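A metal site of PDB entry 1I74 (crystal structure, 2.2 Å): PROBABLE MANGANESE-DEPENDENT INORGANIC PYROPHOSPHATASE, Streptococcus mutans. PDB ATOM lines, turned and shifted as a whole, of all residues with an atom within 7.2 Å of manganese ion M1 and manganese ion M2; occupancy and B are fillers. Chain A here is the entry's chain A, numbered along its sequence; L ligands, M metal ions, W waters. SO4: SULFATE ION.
Within 4 Å of manganese ion M2: His 8, Asp 12 and Asp 75. The nearest printed residue that does not touch manganese ion M2 is Ala 15 (4.1 Å).
Water W1 is bound to manganese ion M2, 1.9 Å away. Manganese ion M2 is bound by O1 of the ligand, 2.0 Å away. The side-chain carboxylate (OD2) of Asp 75 is bound to manganese ion M2 (2.1 Å). The side-chain carboxylate (OD2) of Asp 12 binds manganese ion M2. A ring nitrogen (NE2) of His 8 is bound to manganese ion M2 (2.3 Å). Manganese ion M2 is bound by the side-chain carboxylate (OD1) of Asp 12, 2.5 Å away. Manganese ion M2 has six donor atoms within binding distance.
NE2 of His 97 sits close to N of Ala 119 (3.5 Å). OD1 of Asp 14 lies within hydrogen-bond range of N of Ala 119. N of His 8 lies within hydrogen-bond range of ND1 of His 76 (3.4 Å). OD1 of Asp 12 lies close to N of Asp 14 (3.4 Å). OD1 of Asp 14 is in hydrogen-bond range of OG of Ser 120. The side-chain carboxylate (OD2) of Asp 75 sits close to the backbone NH (N) of Ala 15, at 3.4 Å. O of Asp 14 is in hydrogen-bond range of OG of Ser 18. A ring nitrogen (ND1) of His 98 sits at hydrogen-bond distance from the side-chain carboxylate of Asp 96 (2.6 Å).
Manganese ion M1 is bound by water W1 (2.1 Å), the side-chain carboxylate of Asp 149 (2.1 Å), the side-chain carboxylate of Asp 75 (2.1 Å), an oxygen (O3) of the ligand (2.2 Å), the side-chain carboxylate of Asp 14 (2.3 Å) and a ring nitrogen (NE2) of His 97 (2.4 Å). Manganese ion M1 has six donor atoms within binding distance.
CE1 of His 98 touches manganese ion M1, 3.96 Å away. Five residues have an atom within 4 Å of manganese ion M1: Asp 14, Asp 75, His 97, His 98 and Asp 149. The nearest printed residue that does not touch manganese ion M1 is Ala 119 (4.4 Å).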
ATOM      1  N   HIS A   8      31.374  20.112 -26.409  1.00  0.00           N
ATOM      2  CA  HIS A   8      32.551  19.607 -25.702  1.00  0.00           C
ATOM      3  C   HIS A   8      33.664  18.951 -26.512  1.00  0.00           C
ATOM      4  O   HIS A   8      33.520  18.639 -27.688  1.00  0.00           O
ATOM      5  CB  HIS A   8      32.105  18.634 -24.613  1.00  0.00           C
ATOM      6  CG  HIS A   8      31.303  17.473 -25.123  1.00  0.00           C
ATOM      7  ND1 HIS A   8      31.859  16.469 -25.888  1.00  0.00           N
ATOM      8  CD2 HIS A   8      30.003  17.158 -24.958  1.00  0.00           C
ATOM      9  CE1 HIS A   8      30.926  15.580 -26.174  1.00  0.00           C
ATOM     10  NE2 HIS A   8      29.789  15.967 -25.624  1.00  0.00           N
ATOM     11  N   GLN A   9      34.805  18.770 -25.846  1.00  0.00           N
ATOM     12  CA  GLN A   9      35.972  18.117 -26.436  1.00  0.00           C
ATOM     13  C   GLN A   9      35.489  16.720 -26.823  1.00  0.00           C
ATOM     14  O   GLN A   9      34.569  16.186 -26.194  1.00  0.00           O
ATOM     15  CB  GLN A   9      37.092  18.012 -25.402  1.00  0.00           C
ATOM     16  CG  GLN A   9      37.665  19.351 -24.978  1.00  0.00           C
ATOM     17  CD  GLN A   9      38.602  19.929 -26.012  1.00  0.00           C
ATOM     18  OE1 GLN A   9      39.104  21.054 -25.858  1.00  0.00           O
ATOM     19  NE2 GLN A   9      38.872  19.171 -27.069  1.00  0.00           N
ATOM     20  N   ASN A  10      36.119  16.122 -27.816  1.00  0.00           N
ATOM     21  CA  ASN A  10      35.696  14.797 -28.290  1.00  0.00           C
ATOM     22  C   ASN A  10      34.204  14.904 -28.588  1.00  0.00           C
ATOM     23  O   ASN A  10      33.408  14.112 -28.094  1.00  0.00           O
ATOM     24  CB  ASN A  10      35.933  13.719 -27.233  1.00  0.00           C
ATOM     25  CG  ASN A  10      37.394  13.494 -26.955  1.00  0.00           C
ATOM     26  OD1 ASN A  10      38.260  13.897 -27.722  1.00  0.00           O
ATOM     27  ND2 ASN A  10      37.672  12.816 -25.841  1.00  0.00           N
ATOM     28  N   PRO A  11      33.814  15.884 -29.411  1.00  0.00           N
ATOM     29  CA  PRO A  11      32.437  16.158 -29.819  1.00  0.00           C
ATOM     30  C   PRO A  11      31.693  14.904 -30.261  1.00  0.00           C
ATOM     31  O   PRO A  11      32.221  14.122 -31.053  1.00  0.00           O
ATOM     32  CB  PRO A  11      32.595  17.104 -30.999  1.00  0.00           C
ATOM     33  CG  PRO A  11      33.953  17.667 -30.846  1.00  0.00           C
ATOM     34  CD  PRO A  11      34.770  16.567 -30.291  1.00  0.00           C
ATOM     35  N   ASP A  12      30.479  14.723 -29.763  1.00  0.00           N
ATOM     36  CA  ASP A  12      29.677  13.596 -30.194  1.00  0.00           C
ATOM     37  C   ASP A  12      28.573  14.198 -31.065  1.00  0.00           C
ATOM     38  O   ASP A  12      28.603  15.400 -31.359  1.00  0.00           O
ATOM     39  CB  ASP A  12      29.097  12.840 -28.996  1.00  0.00           C
ATOM     40  CG  ASP A  12      28.439  13.753 -27.979  1.00  0.00           C
ATOM     41  OD1 ASP A  12      28.036  14.882 -28.343  1.00  0.00           O
ATOM     42  OD2 ASP A  12      28.323  13.315 -26.810  1.00  0.00           O
ATOM     43  N   SER A  13      27.612  13.396 -31.506  1.00  0.00           N
ATOM     44  CA  SER A  13      26.567  13.903 -32.368  1.00  0.00           C
ATOM     45  C   SER A  13      25.715  15.020 -31.758  1.00  0.00           C
ATOM     46  O   SER A  13      25.409  16.018 -32.427  1.00  0.00           O
ATOM     47  CB  SER A  13      25.656  12.755 -32.815  1.00  0.00           C
ATOM     48  OG  SER A  13      26.346  11.884 -33.688  1.00  0.00           O
ATOM     49  N   ASP A  14      25.351  14.870 -30.497  1.00  0.00           N
ATOM     50  CA  ASP A  14      24.547  15.874 -29.825  1.00  0.00           C
ATOM     51  C   ASP A  14      25.324  17.183 -29.697  1.00  0.00           C
ATOM     52  O   ASP A  14      24.778  18.260 -29.931  1.00  0.00           O
ATOM     53  CB  ASP A  14      24.117  15.351 -28.463  1.00  0.00           C
ATOM     54  CG  ASP A  14      23.145  16.272 -27.756  1.00  0.00           C
ATOM     55  OD1 ASP A  14      22.206  16.767 -28.411  1.00  0.00           O
ATOM     56  OD2 ASP A  14      23.325  16.501 -26.551  1.00  0.00           O
ATOM     57  N   ALA A  15      26.601  17.088 -29.355  1.00  0.00           N
ATOM     58  CA  ALA A  15      27.433  18.262 -29.216  1.00  0.00           C
ATOM     59  C   ALA A  15      27.480  19.053 -30.519  1.00  0.00           C
ATOM     60  O   ALA A  15      27.247  20.260 -30.540  1.00  0.00           O
ATOM     61  CB  ALA A  15      28.849  17.865 -28.808  1.00  0.00           C
ATOM     62  N   ILE A  16      27.791  18.360 -31.616  1.00  0.00           N
ATOM     63  CA  ILE A  16      27.873  18.997 -32.919  1.00  0.00           C
ATOM     64  C   ILE A  16      26.498  19.489 -33.381  1.00  0.00           C
ATOM     65  O   ILE A  16      26.351  20.634 -33.778  1.00  0.00           O
ATOM     66  CB  ILE A  16      28.463  18.029 -33.984  1.00  0.00           C
ATOM     67  CG1 ILE A  16      29.902  17.637 -33.633  1.00  0.00           C
ATOM     68  CG2 ILE A  16      28.466  18.710 -35.362  1.00  0.00           C
ATOM     69  CD1 ILE A  16      30.873  18.815 -33.586  1.00  0.00           C
ATOM     70  N   SER A  18      23.673  20.136 -31.687  1.00  0.00           N
ATOM     71  CA  SER A  18      23.135  21.221 -30.883  1.00  0.00           C
ATOM     72  C   SER A  18      23.888  22.529 -31.134  1.00  0.00           C
ATOM     73  O   SER A  18      23.278  23.589 -31.171  1.00  0.00           O
ATOM     74  CB  SER A  18      23.179  20.871 -29.390  1.00  0.00           C
ATOM     75  OG  SER A  18      24.504  20.807 -28.893  1.00  0.00           O
ATOM     76  N   THR A  74      27.317  24.544 -25.705  1.00  0.00           N
ATOM     77  CA  THR A  74      26.157  23.663 -25.813  1.00  0.00           C
ATOM     78  C   THR A  74      26.601  22.249 -25.433  1.00  0.00           C
ATOM     79  O   THR A  74      27.743  21.863 -25.687  1.00  0.00           O
ATOM     80  CB  THR A  74      25.544  23.596 -27.250  1.00  0.00           C
ATOM     81  OG1 THR A  74      26.498  23.031 -28.154  1.00  0.00           O
ATOM     82  CG2 THR A  74      25.127  24.974 -27.716  1.00  0.00           C
ATOM     83  N   ASP A  75      25.698  21.502 -24.797  1.00  0.00           N
ATOM     84  CA  ASP A  75      25.952  20.126 -24.430  1.00  0.00           C
ATOM     85  C   ASP A  75      27.083  19.929 -23.404  1.00  0.00           C
ATOM     86  O   ASP A  75      27.649  18.845 -23.298  1.00  0.00           O
ATOM     87  CB  ASP A  75      26.215  19.320 -25.710  1.00  0.00           C
ATOM     88  CG  ASP A  75      26.273  17.826 -25.476  1.00  0.00           C
ATOM     89  OD1 ASP A  75      25.420  17.300 -24.725  1.00  0.00           O
ATOM     90  OD2 ASP A  75      27.158  17.170 -26.050  1.00  0.00           O
ATOM     91  N   HIS A  76      27.396  20.983 -22.666  1.00  0.00           N
ATOM     92  CA  HIS A  76      28.427  20.936 -21.633  1.00  0.00           C
ATOM     93  C   HIS A  76      28.559  22.304 -20.987  1.00  0.00           C
ATOM     94  O   HIS A  76      28.159  23.315 -21.561  1.00  0.00           O
ATOM     95  CB  HIS A  76      29.782  20.547 -22.215  1.00  0.00           C
ATOM     96  CG  HIS A  76      30.450  21.652 -22.981  1.00  0.00           C
ATOM     97  ND1 HIS A  76      29.937  22.169 -24.153  1.00  0.00           N
ATOM     98  CD2 HIS A  76      31.588  22.340 -22.727  1.00  0.00           C
ATOM     99  CE1 HIS A  76      30.729  23.134 -24.583  1.00  0.00           C
ATOM    100  NE2 HIS A  76      31.739  23.263 -23.744  1.00  0.00           N
ATOM    101  N   ASP A  96      22.443  23.308 -22.217  1.00  0.00           N
ATOM    102  CA  ASP A  96      22.963  22.006 -21.871  1.00  0.00           C
ATOM    103  C   ASP A  96      21.986  21.173 -21.049  1.00  0.00           C
ATOM    104  O   ASP A  96      21.000  21.695 -20.537  1.00  0.00           O
ATOM    105  CB  ASP A  96      24.283  22.233 -21.122  1.00  0.00           C
ATOM    106  CG  ASP A  96      24.979  20.956 -20.754  1.00  0.00           C
ATOM    107  OD1 ASP A  96      24.849  19.976 -21.493  1.00  0.00           O
ATOM    108  OD2 ASP A  96      25.676  20.950 -19.729  1.00  0.00           O
ATOM    109  N   HIS A  97      22.265  19.885 -20.922  1.00  0.00           N
ATOM    110  CA  HIS A  97      21.427  18.997 -20.140  1.00  0.00           C
ATOM    111  C   HIS A  97      22.206  18.200 -19.108  1.00  0.00           C
ATOM    112  O   HIS A  97      21.807  17.096 -18.719  1.00  0.00           O
ATOM    113  CB  HIS A  97      20.625  18.053 -21.046  1.00  0.00           C
ATOM    114  CG  HIS A  97      21.457  17.140 -21.887  1.00  0.00           C
ATOM    115  ND1 HIS A  97      21.201  15.793 -21.987  1.00  0.00           N
ATOM    116  CD2 HIS A  97      22.515  17.384 -22.697  1.00  0.00           C
ATOM    117  CE1 HIS A  97      22.070  15.249 -22.827  1.00  0.00           C
ATOM    118  NE2 HIS A  97      22.879  16.193 -23.269  1.00  0.00           N
ATOM    119  N   HIS A  98      23.333  18.745 -18.660  1.00  0.00           N
ATOM    120  CA  HIS A  98      24.150  18.083 -17.675  1.00  0.00           C
ATOM    121  C   HIS A  98      24.118  18.829 -16.355  1.00  0.00           C
ATOM    122  O   HIS A  98      23.660  19.980 -16.284  1.00  0.00           O
ATOM    123  CB  HIS A  98      25.606  17.992 -18.118  1.00  0.00           C
ATOM    124  CG  HIS A  98      25.805  17.174 -19.354  1.00  0.00           C
ATOM    125  ND1 HIS A  98      25.690  17.710 -20.614  1.00  0.00           N
ATOM    126  CD2 HIS A  98      26.131  15.871 -19.514  1.00  0.00           C
ATOM    127  CE1 HIS A  98      25.929  16.770 -21.508  1.00  0.00           C
ATOM    128  NE2 HIS A  98      26.209  15.642 -20.867  1.00  0.00           N
ATOM    129  N   VAL A 116      16.826  16.869 -19.657  1.00  0.00           N
ATOM    130  CA  VAL A 116      16.279  16.017 -20.698  1.00  0.00           C
ATOM    131  C   VAL A 116      17.324  15.141 -21.365  1.00  0.00           C
ATOM    132  O   VAL A 116      18.499  15.176 -21.016  1.00  0.00           O
ATOM    133  CB  VAL A 116      15.576  16.845 -21.793  1.00  0.00           C
ATOM    134  CG1 VAL A 116      14.328  17.495 -21.205  1.00  0.00           C
ATOM    135  CG2 VAL A 116      16.513  17.893 -22.354  1.00  0.00           C
ATOM    136  N   GLY A 117      16.865  14.373 -22.349  1.00  0.00           N
ATOM    137  CA  GLY A 117      17.719  13.443 -23.057  1.00  0.00           C
ATOM    138  C   GLY A 117      18.868  13.958 -23.908  1.00  0.00           C
ATOM    139  O   GLY A 117      19.850  13.249 -24.053  1.00  0.00           O
ATOM    140  N   SER A 118      18.751  15.154 -24.480  1.00  0.00           N
ATOM    141  CA  SER A 118      19.833  15.706 -25.293  1.00  0.00           C
ATOM    142  C   SER A 118      19.789  17.228 -25.298  1.00  0.00           C
ATOM    143  O   SER A 118      18.748  17.817 -25.014  1.00  0.00           O
ATOM    144  CB  SER A 118      19.751  15.207 -26.742  1.00  0.00           C
ATOM    145  OG  SER A 118      18.699  15.831 -27.466  1.00  0.00           O
ATOM    146  N   ALA A 119      20.922  17.855 -25.595  1.00  0.00           N
ATOM    147  CA  ALA A 119      20.986  19.304 -25.668  1.00  0.00           C
ATOM    148  C   ALA A 119      20.215  19.731 -26.908  1.00  0.00           C
ATOM    149  O   ALA A 119      19.634  20.808 -26.952  1.00  0.00           O
ATOM    150  CB  ALA A 119      22.432  19.770 -25.746  1.00  0.00           C
ATOM    151  N   SER A 120      20.220  18.878 -27.929  1.00  0.00           N
ATOM    152  CA  SER A 120      19.502  19.150 -29.157  1.00  0.00           C
ATOM    153  C   SER A 120      18.009  19.269 -28.880  1.00  0.00           C
ATOM    154  O   SER A 120      17.315  20.043 -29.518  1.00  0.00           O
ATOM    155  CB  SER A 120      19.745  18.034 -30.173  1.00  0.00           C
ATOM    156  OG  SER A 120      21.062  18.094 -30.679  1.00  0.00           O
ATOM    157  N   GLY A 145      21.338  14.158 -32.868  1.00  0.00           N
ATOM    158  CA  GLY A 145      21.902  14.376 -31.545  1.00  0.00           C
ATOM    159  C   GLY A 145      21.069  13.679 -30.483  1.00  0.00           C
ATOM    160  O   GLY A 145      21.598  13.031 -29.583  1.00  0.00           O
ATOM    161  N   ASP A 149      22.301  10.446 -28.170  1.00  0.00           N
ATOM    162  CA  ASP A 149      22.337  10.486 -26.718  1.00  0.00           C
ATOM    163  C   ASP A 149      21.395   9.504 -26.026  1.00  0.00           C
ATOM    164  O   ASP A 149      21.684   9.046 -24.925  1.00  0.00           O
ATOM    165  CB  ASP A 149      22.032  11.889 -26.237  1.00  0.00           C
ATOM    166  CG  ASP A 149      23.265  12.747 -26.059  1.00  0.00           C
ATOM    167  OD1 ASP A 149      24.299  12.447 -26.681  1.00  0.00           O
ATOM    168  OD2 ASP A 149      23.196  13.736 -25.301  1.00  0.00           O
ATOM    169  N   ASP A 203      34.945   8.856 -27.497  1.00  0.00           N
ATOM    170  CA  ASP A 203      33.919   9.445 -26.663  1.00  0.00           C
ATOM    171  C   ASP A 203      34.275   9.175 -25.209  1.00  0.00           C
ATOM    172  O   ASP A 203      33.757   8.241 -24.591  1.00  0.00           O
ATOM    173  CB  ASP A 203      32.581   8.821 -27.044  1.00  0.00           C
ATOM    174  CG  ASP A 203      31.424   9.389 -26.288  1.00  0.00           C
ATOM    175  OD1 ASP A 203      31.590  10.433 -25.638  1.00  0.00           O
ATOM    176  OD2 ASP A 203      30.340   8.783 -26.375  1.00  0.00           O
ATOM    177  N   LYS A 205      35.414  11.017 -21.220  1.00  0.00           N
ATOM    178  CA  LYS A 205      35.478  12.141 -20.299  1.00  0.00           C
ATOM    179  C   LYS A 205      36.211  11.719 -19.036  1.00  0.00           C
ATOM    180  O   LYS A 205      36.356  10.519 -18.777  1.00  0.00           O
ATOM    181  CB  LYS A 205      34.070  12.618 -19.910  1.00  0.00           C
ATOM    182  CG  LYS A 205      33.212  13.006 -21.070  1.00  0.00           C
ATOM    183  CD  LYS A 205      31.855  13.590 -20.637  1.00  0.00           C
ATOM    184  CE  LYS A 205      30.933  12.532 -20.043  1.00  0.00           C
ATOM    185  NZ  LYS A 205      29.503  12.976 -20.040  1.00  0.00           N
ATOM    186  N   ARG A 295      26.372   5.754 -19.921  1.00  0.00           N
ATOM    187  CA  ARG A 295      27.501   5.983 -19.054  1.00  0.00           C
ATOM    188  C   ARG A 295      27.062   6.812 -17.848  1.00  0.00           C
ATOM    189  O   ARG A 295      27.271   6.403 -16.706  1.00  0.00           O
ATOM    190  CB  ARG A 295      28.636   6.694 -19.803  1.00  0.00           C
ATOM    191  CG  ARG A 295      29.806   7.141 -18.919  1.00  0.00           C
ATOM    192  CD  ARG A 295      30.981   7.685 -19.734  1.00  0.00           C
ATOM    193  NE  ARG A 295      30.563   8.724 -20.674  1.00  0.00           N
ATOM    194  CZ  ARG A 295      31.227   9.042 -21.792  1.00  0.00           C
ATOM    195  NH1 ARG A 295      32.352   8.404 -22.103  1.00  0.00           N
ATOM    196  NH2 ARG A 295      30.756   9.980 -22.602  1.00  0.00           N
ATOM    197  N   LYS A 296      26.415   7.948 -18.103  1.00  0.00           N
ATOM    198  CA  LYS A 296      26.000   8.832 -17.005  1.00  0.00           C
ATOM    199  C   LYS A 296      25.032   8.225 -16.000  1.00  0.00           C
ATOM    200  O   LYS A 296      25.078   8.567 -14.816  1.00  0.00           O
ATOM    201  CB  LYS A 296      25.403  10.133 -17.551  1.00  0.00           C
ATOM    202  CG  LYS A 296      24.014  10.007 -18.175  1.00  0.00           C
ATOM    203  CD  LYS A 296      23.534  11.347 -18.735  1.00  0.00           C
ATOM    204  CE  LYS A 296      23.443  12.451 -17.660  1.00  0.00           C
ATOM    205  NZ  LYS A 296      23.231  13.815 -18.270  1.00  0.00           N
HETATM  206  S   SO4 L   1      26.681  13.619 -23.292  1.00  0.00           S
HETATM  207  O1  SO4 L   1      27.648  14.415 -24.046  1.00  0.00           O
HETATM  208  O2  SO4 L   1      27.166  13.414 -21.907  1.00  0.00           O
HETATM  209  O3  SO4 L   1      25.382  14.332 -23.282  1.00  0.00           O
HETATM  210  O4  SO4 L   1      26.529  12.322 -23.956  1.00  0.00           O
HETATM  211 MN    MN M   1      24.478  15.390 -24.921  1.00  0.00          MN
HETATM  212 MN    MN M   2      27.635  15.122 -25.871  1.00  0.00          MN
HETATM  213 MG    MG M   3      27.140  10.527 -24.214  1.00  0.00          MG
HETATM  214  O   HOH W   1      25.844  14.570 -26.255  1.00  0.00           O
